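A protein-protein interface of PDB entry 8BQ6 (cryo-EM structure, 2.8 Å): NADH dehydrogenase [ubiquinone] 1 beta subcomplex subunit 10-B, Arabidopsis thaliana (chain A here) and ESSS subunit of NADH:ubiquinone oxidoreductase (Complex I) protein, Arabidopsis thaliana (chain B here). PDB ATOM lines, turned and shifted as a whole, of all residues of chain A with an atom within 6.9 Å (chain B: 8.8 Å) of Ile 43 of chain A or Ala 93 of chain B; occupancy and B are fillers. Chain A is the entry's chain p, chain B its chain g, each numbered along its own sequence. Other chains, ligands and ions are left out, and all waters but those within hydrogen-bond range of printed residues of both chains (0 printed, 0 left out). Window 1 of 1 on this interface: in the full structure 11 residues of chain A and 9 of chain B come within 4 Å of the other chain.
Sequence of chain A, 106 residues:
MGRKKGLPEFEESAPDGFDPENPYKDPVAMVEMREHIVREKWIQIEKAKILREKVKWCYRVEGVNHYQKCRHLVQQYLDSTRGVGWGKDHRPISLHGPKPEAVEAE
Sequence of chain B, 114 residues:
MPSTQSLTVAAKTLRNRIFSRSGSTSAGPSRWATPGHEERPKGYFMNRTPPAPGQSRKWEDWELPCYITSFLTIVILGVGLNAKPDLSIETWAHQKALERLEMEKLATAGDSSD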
ATOM      1  N   LEU A   7      -2.128  21.077 -23.692  1.00  0.00           N
ATOM      2  CA  LEU A   7      -0.886  21.560 -23.125  1.00  0.00           C
ATOM      3  C   LEU A   7      -0.687  23.034 -23.477  1.00  0.00           C
ATOM      4  O   LEU A   7      -1.172  23.504 -24.509  1.00  0.00           O
ATOM      5  CB  LEU A   7       0.281  20.727 -23.642  1.00  0.00           C
ATOM      6  CG  LEU A   7       1.319  20.273 -22.616  1.00  0.00           C
ATOM      7  CD1 LEU A   7       0.713  19.303 -21.618  1.00  0.00           C
ATOM      8  CD2 LEU A   7       2.502  19.645 -23.323  1.00  0.00           C
ATOM      9  N   HIS A  36      11.487  33.075 -22.370  1.00  0.00           N
ATOM     10  CA  HIS A  36      11.940  32.115 -23.371  1.00  0.00           C
ATOM     11  C   HIS A  36      13.180  31.368 -22.897  1.00  0.00           C
ATOM     12  O   HIS A  36      13.317  30.164 -23.141  1.00  0.00           O
ATOM     13  CB  HIS A  36      12.203  32.835 -24.694  1.00  0.00           C
ATOM     14  CG  HIS A  36      12.781  31.959 -25.762  1.00  0.00           C
ATOM     15  ND1 HIS A  36      11.999  31.256 -26.652  1.00  0.00           N
ATOM     16  CD2 HIS A  36      14.065  31.690 -26.096  1.00  0.00           C
ATOM     17  CE1 HIS A  36      12.777  30.584 -27.482  1.00  0.00           C
ATOM     18  NE2 HIS A  36      14.035  30.831 -27.167  1.00  0.00           N
ATOM     19  N   ILE A  37      14.096  32.065 -22.222  1.00  0.00           N
ATOM     20  CA  ILE A  37      15.292  31.409 -21.697  1.00  0.00           C
ATOM     21  C   ILE A  37      14.923  30.430 -20.593  1.00  0.00           C
ATOM     22  O   ILE A  37      15.496  29.338 -20.497  1.00  0.00           O
ATOM     23  CB  ILE A  37      16.306  32.451 -21.196  1.00  0.00           C
ATOM     24  CG1 ILE A  37      16.879  33.249 -22.360  1.00  0.00           C
ATOM     25  CG2 ILE A  37      17.436  31.770 -20.448  1.00  0.00           C
ATOM     26  CD1 ILE A  37      17.504  34.537 -21.920  1.00  0.00           C
ATOM     27  N   VAL A  38      13.979  30.813 -19.728  1.00  0.00           N
ATOM     28  CA  VAL A  38      13.539  29.909 -18.670  1.00  0.00           C
ATOM     29  C   VAL A  38      12.972  28.634 -19.275  1.00  0.00           C
ATOM     30  O   VAL A  38      13.303  27.522 -18.846  1.00  0.00           O
ATOM     31  CB  VAL A  38      12.510  30.606 -17.762  1.00  0.00           C
ATOM     32  CG1 VAL A  38      11.721  29.579 -16.968  1.00  0.00           C
ATOM     33  CG2 VAL A  38      13.196  31.597 -16.838  1.00  0.00           C
ATOM     34  N   ARG A  39      12.127  28.779 -20.295  1.00  0.00           N
ATOM     35  CA  ARG A  39      11.549  27.615 -20.954  1.00  0.00           C
ATOM     36  C   ARG A  39      12.621  26.783 -21.639  1.00  0.00           C
ATOM     37  O   ARG A  39      12.574  25.548 -21.610  1.00  0.00           O
ATOM     38  CB  ARG A  39      10.495  28.060 -21.959  1.00  0.00           C
ATOM     39  CG  ARG A  39       9.190  28.466 -21.327  1.00  0.00           C
ATOM     40  CD  ARG A  39       8.197  28.830 -22.395  1.00  0.00           C
ATOM     41  NE  ARG A  39       7.838  30.239 -22.351  1.00  0.00           N
ATOM     42  CZ  ARG A  39       8.025  31.088 -23.351  1.00  0.00           C
ATOM     43  NH1 ARG A  39       8.613  30.712 -24.476  1.00  0.00           N
ATOM     44  NH2 ARG A  39       7.610  32.344 -23.222  1.00  0.00           N
ATOM     45  N   GLU A  40      13.589  27.443 -22.276  1.00  0.00           N
ATOM     46  CA  GLU A  40      14.669  26.714 -22.926  1.00  0.00           C
ATOM     47  C   GLU A  40      15.508  25.958 -21.904  1.00  0.00           C
ATOM     48  O   GLU A  40      15.866  24.795 -22.118  1.00  0.00           O
ATOM     49  CB  GLU A  40      15.531  27.678 -23.739  1.00  0.00           C
ATOM     50  CG  GLU A  40      15.905  27.146 -25.107  1.00  0.00           C
ATOM     51  CD  GLU A  40      14.692  26.870 -25.969  1.00  0.00           C
ATOM     52  OE1 GLU A  40      14.786  26.015 -26.874  1.00  0.00           O
ATOM     53  OE2 GLU A  40      13.645  27.514 -25.750  1.00  0.00           O
ATOM     54  N   LYS A  41      15.810  26.597 -20.772  1.00  0.00           N
ATOM     55  CA  LYS A  41      16.597  25.927 -19.744  1.00  0.00           C
ATOM     56  C   LYS A  41      15.858  24.718 -19.190  1.00  0.00           C
ATOM     57  O   LYS A  41      16.477  23.694 -18.876  1.00  0.00           O
ATOM     58  CB  LYS A  41      16.955  26.903 -18.626  1.00  0.00           C
ATOM     59  CG  LYS A  41      18.041  27.875 -19.022  1.00  0.00           C
ATOM     60  CD  LYS A  41      18.465  28.793 -17.894  1.00  0.00           C
ATOM     61  CE  LYS A  41      19.633  29.651 -18.358  1.00  0.00           C
ATOM     62  NZ  LYS A  41      20.466  30.190 -17.251  1.00  0.00           N
ATOM     63  N   TRP A  42      14.533  24.809 -19.074  1.00  0.00           N
ATOM     64  CA  TRP A  42      13.760  23.679 -18.571  1.00  0.00           C
ATOM     65  C   TRP A  42      13.748  22.523 -19.561  1.00  0.00           C
ATOM     66  O   TRP A  42      13.602  21.362 -19.161  1.00  0.00           O
ATOM     67  CB  TRP A  42      12.336  24.118 -18.241  1.00  0.00           C
ATOM     68  CG  TRP A  42      12.201  24.610 -16.842  1.00  0.00           C
ATOM     69  CD1 TRP A  42      12.103  25.904 -16.437  1.00  0.00           C
ATOM     70  CD2 TRP A  42      12.165  23.814 -15.653  1.00  0.00           C
ATOM     71  NE1 TRP A  42      12.003  25.967 -15.070  1.00  0.00           N
ATOM     72  CE2 TRP A  42      12.042  24.696 -14.565  1.00  0.00           C
ATOM     73  CE3 TRP A  42      12.228  22.441 -15.405  1.00  0.00           C
ATOM     74  CZ2 TRP A  42      11.973  24.252 -13.250  1.00  0.00           C
ATOM     75  CZ3 TRP A  42      12.162  22.003 -14.100  1.00  0.00           C
ATOM     76  CH2 TRP A  42      12.033  22.905 -13.039  1.00  0.00           C
ATOM     77  N   ILE A  43      13.884  22.816 -20.855  1.00  0.00           N
ATOM     78  CA  ILE A  43      13.944  21.749 -21.851  1.00  0.00           C
ATOM     79  C   ILE A  43      15.226  20.943 -21.689  1.00  0.00           C
ATOM     80  O   ILE A  43      15.214  19.709 -21.758  1.00  0.00           O
ATOM     81  CB  ILE A  43      13.804  22.327 -23.270  1.00  0.00           C
ATOM     82  CG1 ILE A  43      12.392  22.868 -23.482  1.00  0.00           C
ATOM     83  CG2 ILE A  43      14.091  21.265 -24.311  1.00  0.00           C
ATOM     84  CD1 ILE A  43      12.268  23.787 -24.666  1.00  0.00           C
ATOM     85  N   GLN A  44      16.350  21.624 -21.459  1.00  0.00           N
ATOM     86  CA  GLN A  44      17.598  20.907 -21.228  1.00  0.00           C
ATOM     87  C   GLN A  44      17.571  20.152 -19.908  1.00  0.00           C
ATOM     88  O   GLN A  44      18.193  19.091 -19.782  1.00  0.00           O
ATOM     89  CB  GLN A  44      18.784  21.865 -21.263  1.00  0.00           C
ATOM     90  CG  GLN A  44      18.990  22.515 -22.601  1.00  0.00           C
ATOM     91  CD  GLN A  44      20.337  23.183 -22.708  1.00  0.00           C
ATOM     92  OE1 GLN A  44      20.942  23.551 -21.702  1.00  0.00           O
ATOM     93  NE2 GLN A  44      20.819  23.341 -23.933  1.00  0.00           N
ATOM     94  N   ILE A  45      16.875  20.687 -18.903  1.00  0.00           N
ATOM     95  CA  ILE A  45      16.750  19.954 -17.648  1.00  0.00           C
ATOM     96  C   ILE A  45      16.043  18.630 -17.893  1.00  0.00           C
ATOM     97  O   ILE A  45      16.516  17.566 -17.475  1.00  0.00           O
ATOM     98  CB  ILE A  45      16.030  20.802 -16.583  1.00  0.00           C
ATOM     99  CG1 ILE A  45      16.952  21.905 -16.069  1.00  0.00           C
ATOM    100  CG2 ILE A  45      15.605  19.937 -15.419  1.00  0.00           C
ATOM    101  CD1 ILE A  45      16.233  23.170 -15.705  1.00  0.00           C
ATOM    102  N   GLU A  46      14.932  18.667 -18.629  1.00  0.00           N
ATOM    103  CA  GLU A  46      14.234  17.431 -18.957  1.00  0.00           C
ATOM    104  C   GLU A  46      15.075  16.534 -19.857  1.00  0.00           C
ATOM    105  O   GLU A  46      14.950  15.306 -19.796  1.00  0.00           O
ATOM    106  CB  GLU A  46      12.896  17.749 -19.615  1.00  0.00           C
ATOM    107  CG  GLU A  46      11.978  18.593 -18.755  1.00  0.00           C
ATOM    108  CD  GLU A  46      11.433  17.836 -17.564  1.00  0.00           C
ATOM    109  OE1 GLU A  46      10.733  16.828 -17.772  1.00  0.00           O
ATOM    110  OE2 GLU A  46      11.685  18.264 -16.420  1.00  0.00           O
ATOM    111  N   LYS A  47      15.940  17.122 -20.685  1.00  0.00           N
ATOM    112  CA  LYS A  47      16.834  16.322 -21.517  1.00  0.00           C
ATOM    113  C   LYS A  47      17.741  15.445 -20.662  1.00  0.00           C
ATOM    114  O   LYS A  47      17.863  14.239 -20.904  1.00  0.00           O
ATOM    115  CB  LYS A  47      17.669  17.232 -22.415  1.00  0.00           C
ATOM    116  CG  LYS A  47      18.525  16.498 -23.418  1.00  0.00           C
ATOM    117  CD  LYS A  47      19.658  17.372 -23.924  1.00  0.00           C
ATOM    118  CE  LYS A  47      19.136  18.691 -24.473  1.00  0.00           C
ATOM    119  NZ  LYS A  47      20.208  19.505 -25.105  1.00  0.00           N
ATOM    120  N   ALA A  48      18.379  16.034 -19.650  1.00  0.00           N
ATOM    121  CA  ALA A  48      19.254  15.257 -18.780  1.00  0.00           C
ATOM    122  C   ALA A  48      18.476  14.220 -17.982  1.00  0.00           C
ATOM    123  O   ALA A  48      19.014  13.156 -17.663  1.00  0.00           O
ATOM    124  CB  ALA A  48      20.024  16.186 -17.844  1.00  0.00           C
ATOM    125  N   ILE A  50      15.735  12.630 -19.040  1.00  0.00           N
ATOM    126  CA  ILE A  50      15.422  11.530 -19.999  1.00  0.00           C
ATOM    127  C   ILE A  50      16.706  10.715 -20.164  1.00  0.00           C
ATOM    128  O   ILE A  50      16.631   9.471 -20.108  1.00  0.00           O
ATOM    129  CB  ILE A  50      14.929  12.120 -21.337  1.00  0.00           C
ATOM    130  CG1 ILE A  50      13.490  12.633 -21.236  1.00  0.00           C
ATOM    131  CG2 ILE A  50      15.090  11.137 -22.488  1.00  0.00           C
ATOM    132  CD1 ILE A  50      13.118  13.625 -22.313  1.00  0.00           C
ATOM    133  N   LEU B  87      -0.472  21.963 -16.164  1.00  0.00           N
ATOM    134  CA  LEU B  87       0.216  23.026 -16.886  1.00  0.00           C
ATOM    135  C   LEU B  87       1.587  23.337 -16.301  1.00  0.00           C
ATOM    136  O   LEU B  87       2.051  24.475 -16.397  1.00  0.00           O
ATOM    137  CB  LEU B  87      -0.634  24.296 -16.923  1.00  0.00           C
ATOM    138  CG  LEU B  87      -2.113  24.186 -17.290  1.00  0.00           C
ATOM    139  CD1 LEU B  87      -2.859  25.392 -16.776  1.00  0.00           C
ATOM    140  CD2 LEU B  87      -2.275  24.083 -18.788  1.00  0.00           C
ATOM    141  N   SER B  88       2.247  22.357 -15.694  1.00  0.00           N
ATOM    142  CA  SER B  88       3.568  22.609 -15.144  1.00  0.00           C
ATOM    143  C   SER B  88       4.587  22.787 -16.264  1.00  0.00           C
ATOM    144  O   SER B  88       4.457  22.223 -17.353  1.00  0.00           O
ATOM    145  CB  SER B  88       3.984  21.470 -14.213  1.00  0.00           C
ATOM    146  OG  SER B  88       4.228  20.274 -14.930  1.00  0.00           O
ATOM    147  N   ILE B  89       5.602  23.611 -15.990  1.00  0.00           N
ATOM    148  CA  ILE B  89       6.705  23.783 -16.930  1.00  0.00           C
ATOM    149  C   ILE B  89       7.425  22.459 -17.140  1.00  0.00           C
ATOM    150  O   ILE B  89       8.014  22.220 -18.202  1.00  0.00           O
ATOM    151  CB  ILE B  89       7.659  24.885 -16.423  1.00  0.00           C
ATOM    152  CG1 ILE B  89       8.706  25.232 -17.480  1.00  0.00           C
ATOM    153  CG2 ILE B  89       8.340  24.461 -15.133  1.00  0.00           C
ATOM    154  CD1 ILE B  89       8.151  25.993 -18.655  1.00  0.00           C
ATOM    155  N   GLU B  90       7.376  21.573 -16.144  1.00  0.00           N
ATOM    156  CA  GLU B  90       8.017  20.269 -16.261  1.00  0.00           C
ATOM    157  C   GLU B  90       7.301  19.383 -17.275  1.00  0.00           C
ATOM    158  O   GLU B  90       7.945  18.687 -18.068  1.00  0.00           O
ATOM    159  CB  GLU B  90       8.072  19.595 -14.891  1.00  0.00           C
ATOM    160  CG  GLU B  90       8.426  20.544 -13.758  1.00  0.00           C
ATOM    161  CD  GLU B  90       8.096  19.978 -12.393  1.00  0.00           C
ATOM    162  OE1 GLU B  90       7.766  20.771 -11.487  1.00  0.00           O
ATOM    163  OE2 GLU B  90       8.169  18.743 -12.224  1.00  0.00           O
ATOM    164  N   THR B  91       5.967  19.378 -17.259  1.00  0.00           N
ATOM    165  CA  THR B  91       5.244  18.517 -18.192  1.00  0.00           C
ATOM    166  C   THR B  91       5.377  19.023 -19.622  1.00  0.00           C
ATOM    167  O   THR B  91       5.471  18.228 -20.564  1.00  0.00           O
ATOM    168  CB  THR B  91       3.774  18.408 -17.788  1.00  0.00           C
ATOM    169  OG1 THR B  91       3.684  17.826 -16.483  1.00  0.00           O
ATOM    170  CG2 THR B  91       3.011  17.536 -18.768  1.00  0.00           C
ATOM    171  N   TRP B  92       5.400  20.343 -19.800  1.00  0.00           N
ATOM    172  CA  TRP B  92       5.520  20.907 -21.137  1.00  0.00           C
ATOM    173  C   TRP B  92       6.919  20.699 -21.702  1.00  0.00           C
ATOM    174  O   TRP B  92       7.075  20.353 -22.879  1.00  0.00           O
ATOM    175  CB  TRP B  92       5.163  22.389 -21.099  1.00  0.00           C
ATOM    176  CG  TRP B  92       5.492  23.113 -22.347  1.00  0.00           C
ATOM    177  CD1 TRP B  92       4.681  23.281 -23.423  1.00  0.00           C
ATOM    178  CD2 TRP B  92       6.715  23.791 -22.653  1.00  0.00           C
ATOM    179  NE1 TRP B  92       5.322  24.014 -24.388  1.00  0.00           N
ATOM    180  CE2 TRP B  92       6.574  24.341 -23.939  1.00  0.00           C
ATOM    181  CE3 TRP B  92       7.917  23.983 -21.965  1.00  0.00           C
ATOM    182  CZ2 TRP B  92       7.587  25.068 -24.554  1.00  0.00           C
ATOM    183  CZ3 TRP B  92       8.919  24.706 -22.577  1.00  0.00           C
ATOM    184  CH2 TRP B  92       8.749  25.240 -23.858  1.00  0.00           C
ATOM    185  N   ALA B  93       7.947  20.903 -20.879  1.00  0.00           N
ATOM    186  CA  ALA B  93       9.312  20.718 -21.352  1.00  0.00           C
ATOM    187  C   ALA B  93       9.630  19.251 -21.604  1.00  0.00           C
ATOM    188  O   ALA B  93      10.440  18.942 -22.483  1.00  0.00           O
ATOM    189  CB  ALA B  93      10.302  21.310 -20.353  1.00  0.00           C
ATOM    190  N   HIS B  94       9.035  18.354 -20.809  1.00  0.00           N
ATOM    191  CA  HIS B  94       9.254  16.897 -21.014  1.00  0.00           C
ATOM    192  C   HIS B  94       8.845  16.535 -22.436  1.00  0.00           C
ATOM    193  O   HIS B  94       9.667  15.935 -23.150  1.00  0.00           O
ATOM    194  CB  HIS B  94       8.458  16.065 -20.005  1.00  0.00           C
ATOM    195  CG  HIS B  94       8.749  14.606 -20.096  1.00  0.00           C
ATOM    196  ND1 HIS B  94      10.020  14.096 -19.927  1.00  0.00           N
ATOM    197  CD2 HIS B  94       7.947  13.551 -20.355  1.00  0.00           C
ATOM    198  CE1 HIS B  94       9.987  12.787 -20.068  1.00  0.00           C
ATOM    199  NE2 HIS B  94       8.727  12.427 -20.331  1.00  0.00           N
ATOM    200  N   GLN B  95       7.616  16.888 -22.815  1.00  0.00           N
ATOM    201  CA  GLN B  95       7.133  16.617 -24.163  1.00  0.00           C
ATOM    202  C   GLN B  95       8.002  17.304 -25.208  1.00  0.00           C
ATOM    203  O   GLN B  95       8.318  16.717 -26.249  1.00  0.00           O
ATOM    204  CB  GLN B  95       5.684  17.075 -24.284  1.00  0.00           C
ATOM    205  CG  GLN B  95       5.294  17.502 -25.671  1.00  0.00           C
ATOM    206  CD  GLN B  95       4.499  16.438 -26.374  1.00  0.00           C
ATOM    207  OE1 GLN B  95       4.415  15.302 -25.908  1.00  0.00           O
ATOM    208  NE2 GLN B  95       3.905  16.794 -27.503  1.00  0.00           N
ATOM    209  N   LYS B  96       8.390  18.553 -24.944  1.00  0.00           N
ATOM    210  CA  LYS B  96       9.229  19.295 -25.877  1.00  0.00           C
ATOM    211  C   LYS B  96      10.600  18.649 -26.026  1.00  0.00           C
ATOM    212  O   LYS B  96      11.157  18.608 -27.129  1.00  0.00           O
ATOM    213  CB  LYS B  96       9.374  20.738 -25.404  1.00  0.00           C
ATOM    214  CG  LYS B  96       8.277  21.651 -25.880  1.00  0.00           C
ATOM    215  CD  LYS B  96       8.549  22.154 -27.276  1.00  0.00           C
ATOM    216  CE  LYS B  96       7.276  22.683 -27.903  1.00  0.00           C
ATOM    217  NZ  LYS B  96       6.112  21.835 -27.527  1.00  0.00           N
ATOM    218  N   ALA B  97      11.166  18.154 -24.925  1.00  0.00           N
ATOM    219  CA  ALA B  97      12.500  17.568 -24.980  1.00  0.00           C
ATOM    220  C   ALA B  97      12.473  16.200 -25.650  1.00  0.00           C
ATOM    221  O   ALA B  97      13.474  15.763 -26.230  1.00  0.00           O
ATOM    222  CB  ALA B  97      13.090  17.470 -23.573  1.00  0.00           C
ATOM    223  N   LEU B  98      11.326  15.522 -25.564  1.00  0.00           N
ATOM    224  CA  LEU B  98      11.179  14.187 -26.203  1.00  0.00           C
ATOM    225  C   LEU B  98      11.251  14.345 -27.723  1.00  0.00           C
ATOM    226  O   LEU B  98      11.933  13.523 -28.356  1.00  0.00           O
ATOM    227  CB  LEU B  98       9.834  13.588 -25.784  1.00  0.00           C
ATOM    228  CG  LEU B  98       9.877  12.688 -24.552  1.00  0.00           C
ATOM    229  CD1 LEU B  98       8.475  12.429 -24.025  1.00  0.00           C
ATOM    230  CD2 LEU B  98      10.579  11.379 -24.872  1.00  0.00           C
ATOM    231  N   GLU B  99      10.583  15.363 -28.275  1.00  0.00           N
ATOM    232  CA  GLU B  99      10.550  15.545 -29.719  1.00  0.00           C
ATOM    233  C   GLU B  99      11.886  16.029 -30.260  1.00  0.00           C
ATOM    234  O   GLU B  99      12.247  15.699 -31.394  1.00  0.00           O
ATOM    235  CB  GLU B  99       9.442  16.519 -30.093  1.00  0.00           C
ATOM    236  CG  GLU B  99       8.203  15.825 -30.597  1.00  0.00           C
ATOM    237  CD  GLU B  99       6.949  16.486 -30.099  1.00  0.00           C
ATOM    238  OE1 GLU B  99       7.068  17.564 -29.482  1.00  0.00           O
ATOM    239  OE2 GLU B  99       5.854  15.927 -30.311  1.00  0.00           O
ATOM    240  N   ARG B 100      12.620  16.821 -29.480  1.00  0.00           N
ATOM    241  CA  ARG B 100      13.919  17.292 -29.943  1.00  0.00           C
ATOM    242  C   ARG B 100      14.958  16.178 -29.928  1.00  0.00           C
ATOM    243  O   ARG B 100      15.828  16.133 -30.804  1.00  0.00           O
ATOM    244  CB  ARG B 100      14.381  18.475 -29.101  1.00  0.00           C
ATOM    245  CG  ARG B 100      13.716  19.777 -29.489  1.00  0.00           C
ATOM    246  CD  ARG B 100      14.411  20.936 -28.826  1.00  0.00           C
ATOM    247  NE  ARG B 100      13.516  22.073 -28.657  1.00  0.00           N
ATOM    248  CZ  ARG B 100      13.896  23.251 -28.186  1.00  0.00           C
ATOM    249  NH1 ARG B 100      15.143  23.471 -27.804  1.00  0.00           N
ATOM    250  NH2 ARG B 100      13.003  24.231 -28.092  1.00  0.00           N
ATOM    251  N   LEU B 101      14.890  15.275 -28.945  1.00  0.00           N
ATOM    252  CA  LEU B 101      15.753  14.097 -28.981  1.00  0.00           C
ATOM    253  C   LEU B 101      15.295  13.096 -30.030  1.00  0.00           C
ATOM    254  O   LEU B 101      16.114  12.330 -30.550  1.00  0.00           O
ATOM    255  CB  LEU B 101      15.835  13.428 -27.609  1.00  0.00           C
ATOM    256  CG  LEU B 101      17.078  13.842 -26.816  1.00  0.00           C
ATOM    257  CD1 LEU B 101      17.360  15.321 -26.992  1.00  0.00           C
ATOM    258  CD2 LEU B 101      16.993  13.463 -25.345  1.00  0.00           C
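The side-chain carboxylate of Glu 40 of chain A is in salt-bridge range of the guanidinium group of Arg 100 of chain B (2.7 Å).
The side-chain carboxylate of Glu 46 of chain A sits close to the backbone carbonyl oxygen of Glu 90 of chain B (3.4 Å).
CD2 of Leu 7 of chain A touches CA of Trp 92 of chain B, 3.9 Å away.
Arg 39 of chain A touches Ile 89 of chain B (CG to CD1, 3.8 Å).
Trp 42 of chain A touches Ile 89 of chain B.
Ala 93 of chain B touches Trp 42 of chain A.
Ile 43 of chain A touches Trp 92 of chain B.
Ile 43 of chain A touches Ala 93 of chain B.
Ala 97 of chain B touches Ile 43 of chain A.
CB of Ala 93 of chain B touches CG of Glu 46 of chain A (3.6 Å).
Glu 46 of chain A touches Ala 97 of chain B.
CD2 of Leu 101 of chain B touches CG of Lys 47 of chain A (3.9 Å).
Ile 43 of chain A touches just these residues of chain B: Trp 92 (3.9 Å), Ala 93 (3.9 Å), Ala 97 (3.6 Å) and Arg 100 (3.5 Å).
Ala 93 of chain B touches three residues of chain A.
Of the printed residues of chain A, Arg 100 of chain B touches Glu 40 and Ile 43.
Of the printed residues of chain B, Glu 46 of chain A touches Glu 90, Ala 93, His 94 and Ala 97.
Of the printed residues of chain B, Lys 47 of chain A touches Leu 101.
Thr 91 of chain B touches none of the printed residues of chain A.
The nearest printed residue of chain B that does not touch Glu 40 of chain A is Trp 92 of chain B (5.4 Å).
Hydrophobic or aromatic side chains of chain B that line the printed part of chain A: Ile 89, Trp 92, Ala 93, His 94, Ala 97 and Leu 101.
Of the 15 printed residues of chain A, 8 touch a printed residue of chain B.
Hydrophobic or aromatic side chains of chain A that line the printed part of chain B: Leu 7, Trp 42, Ile 43 and Ile 50.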
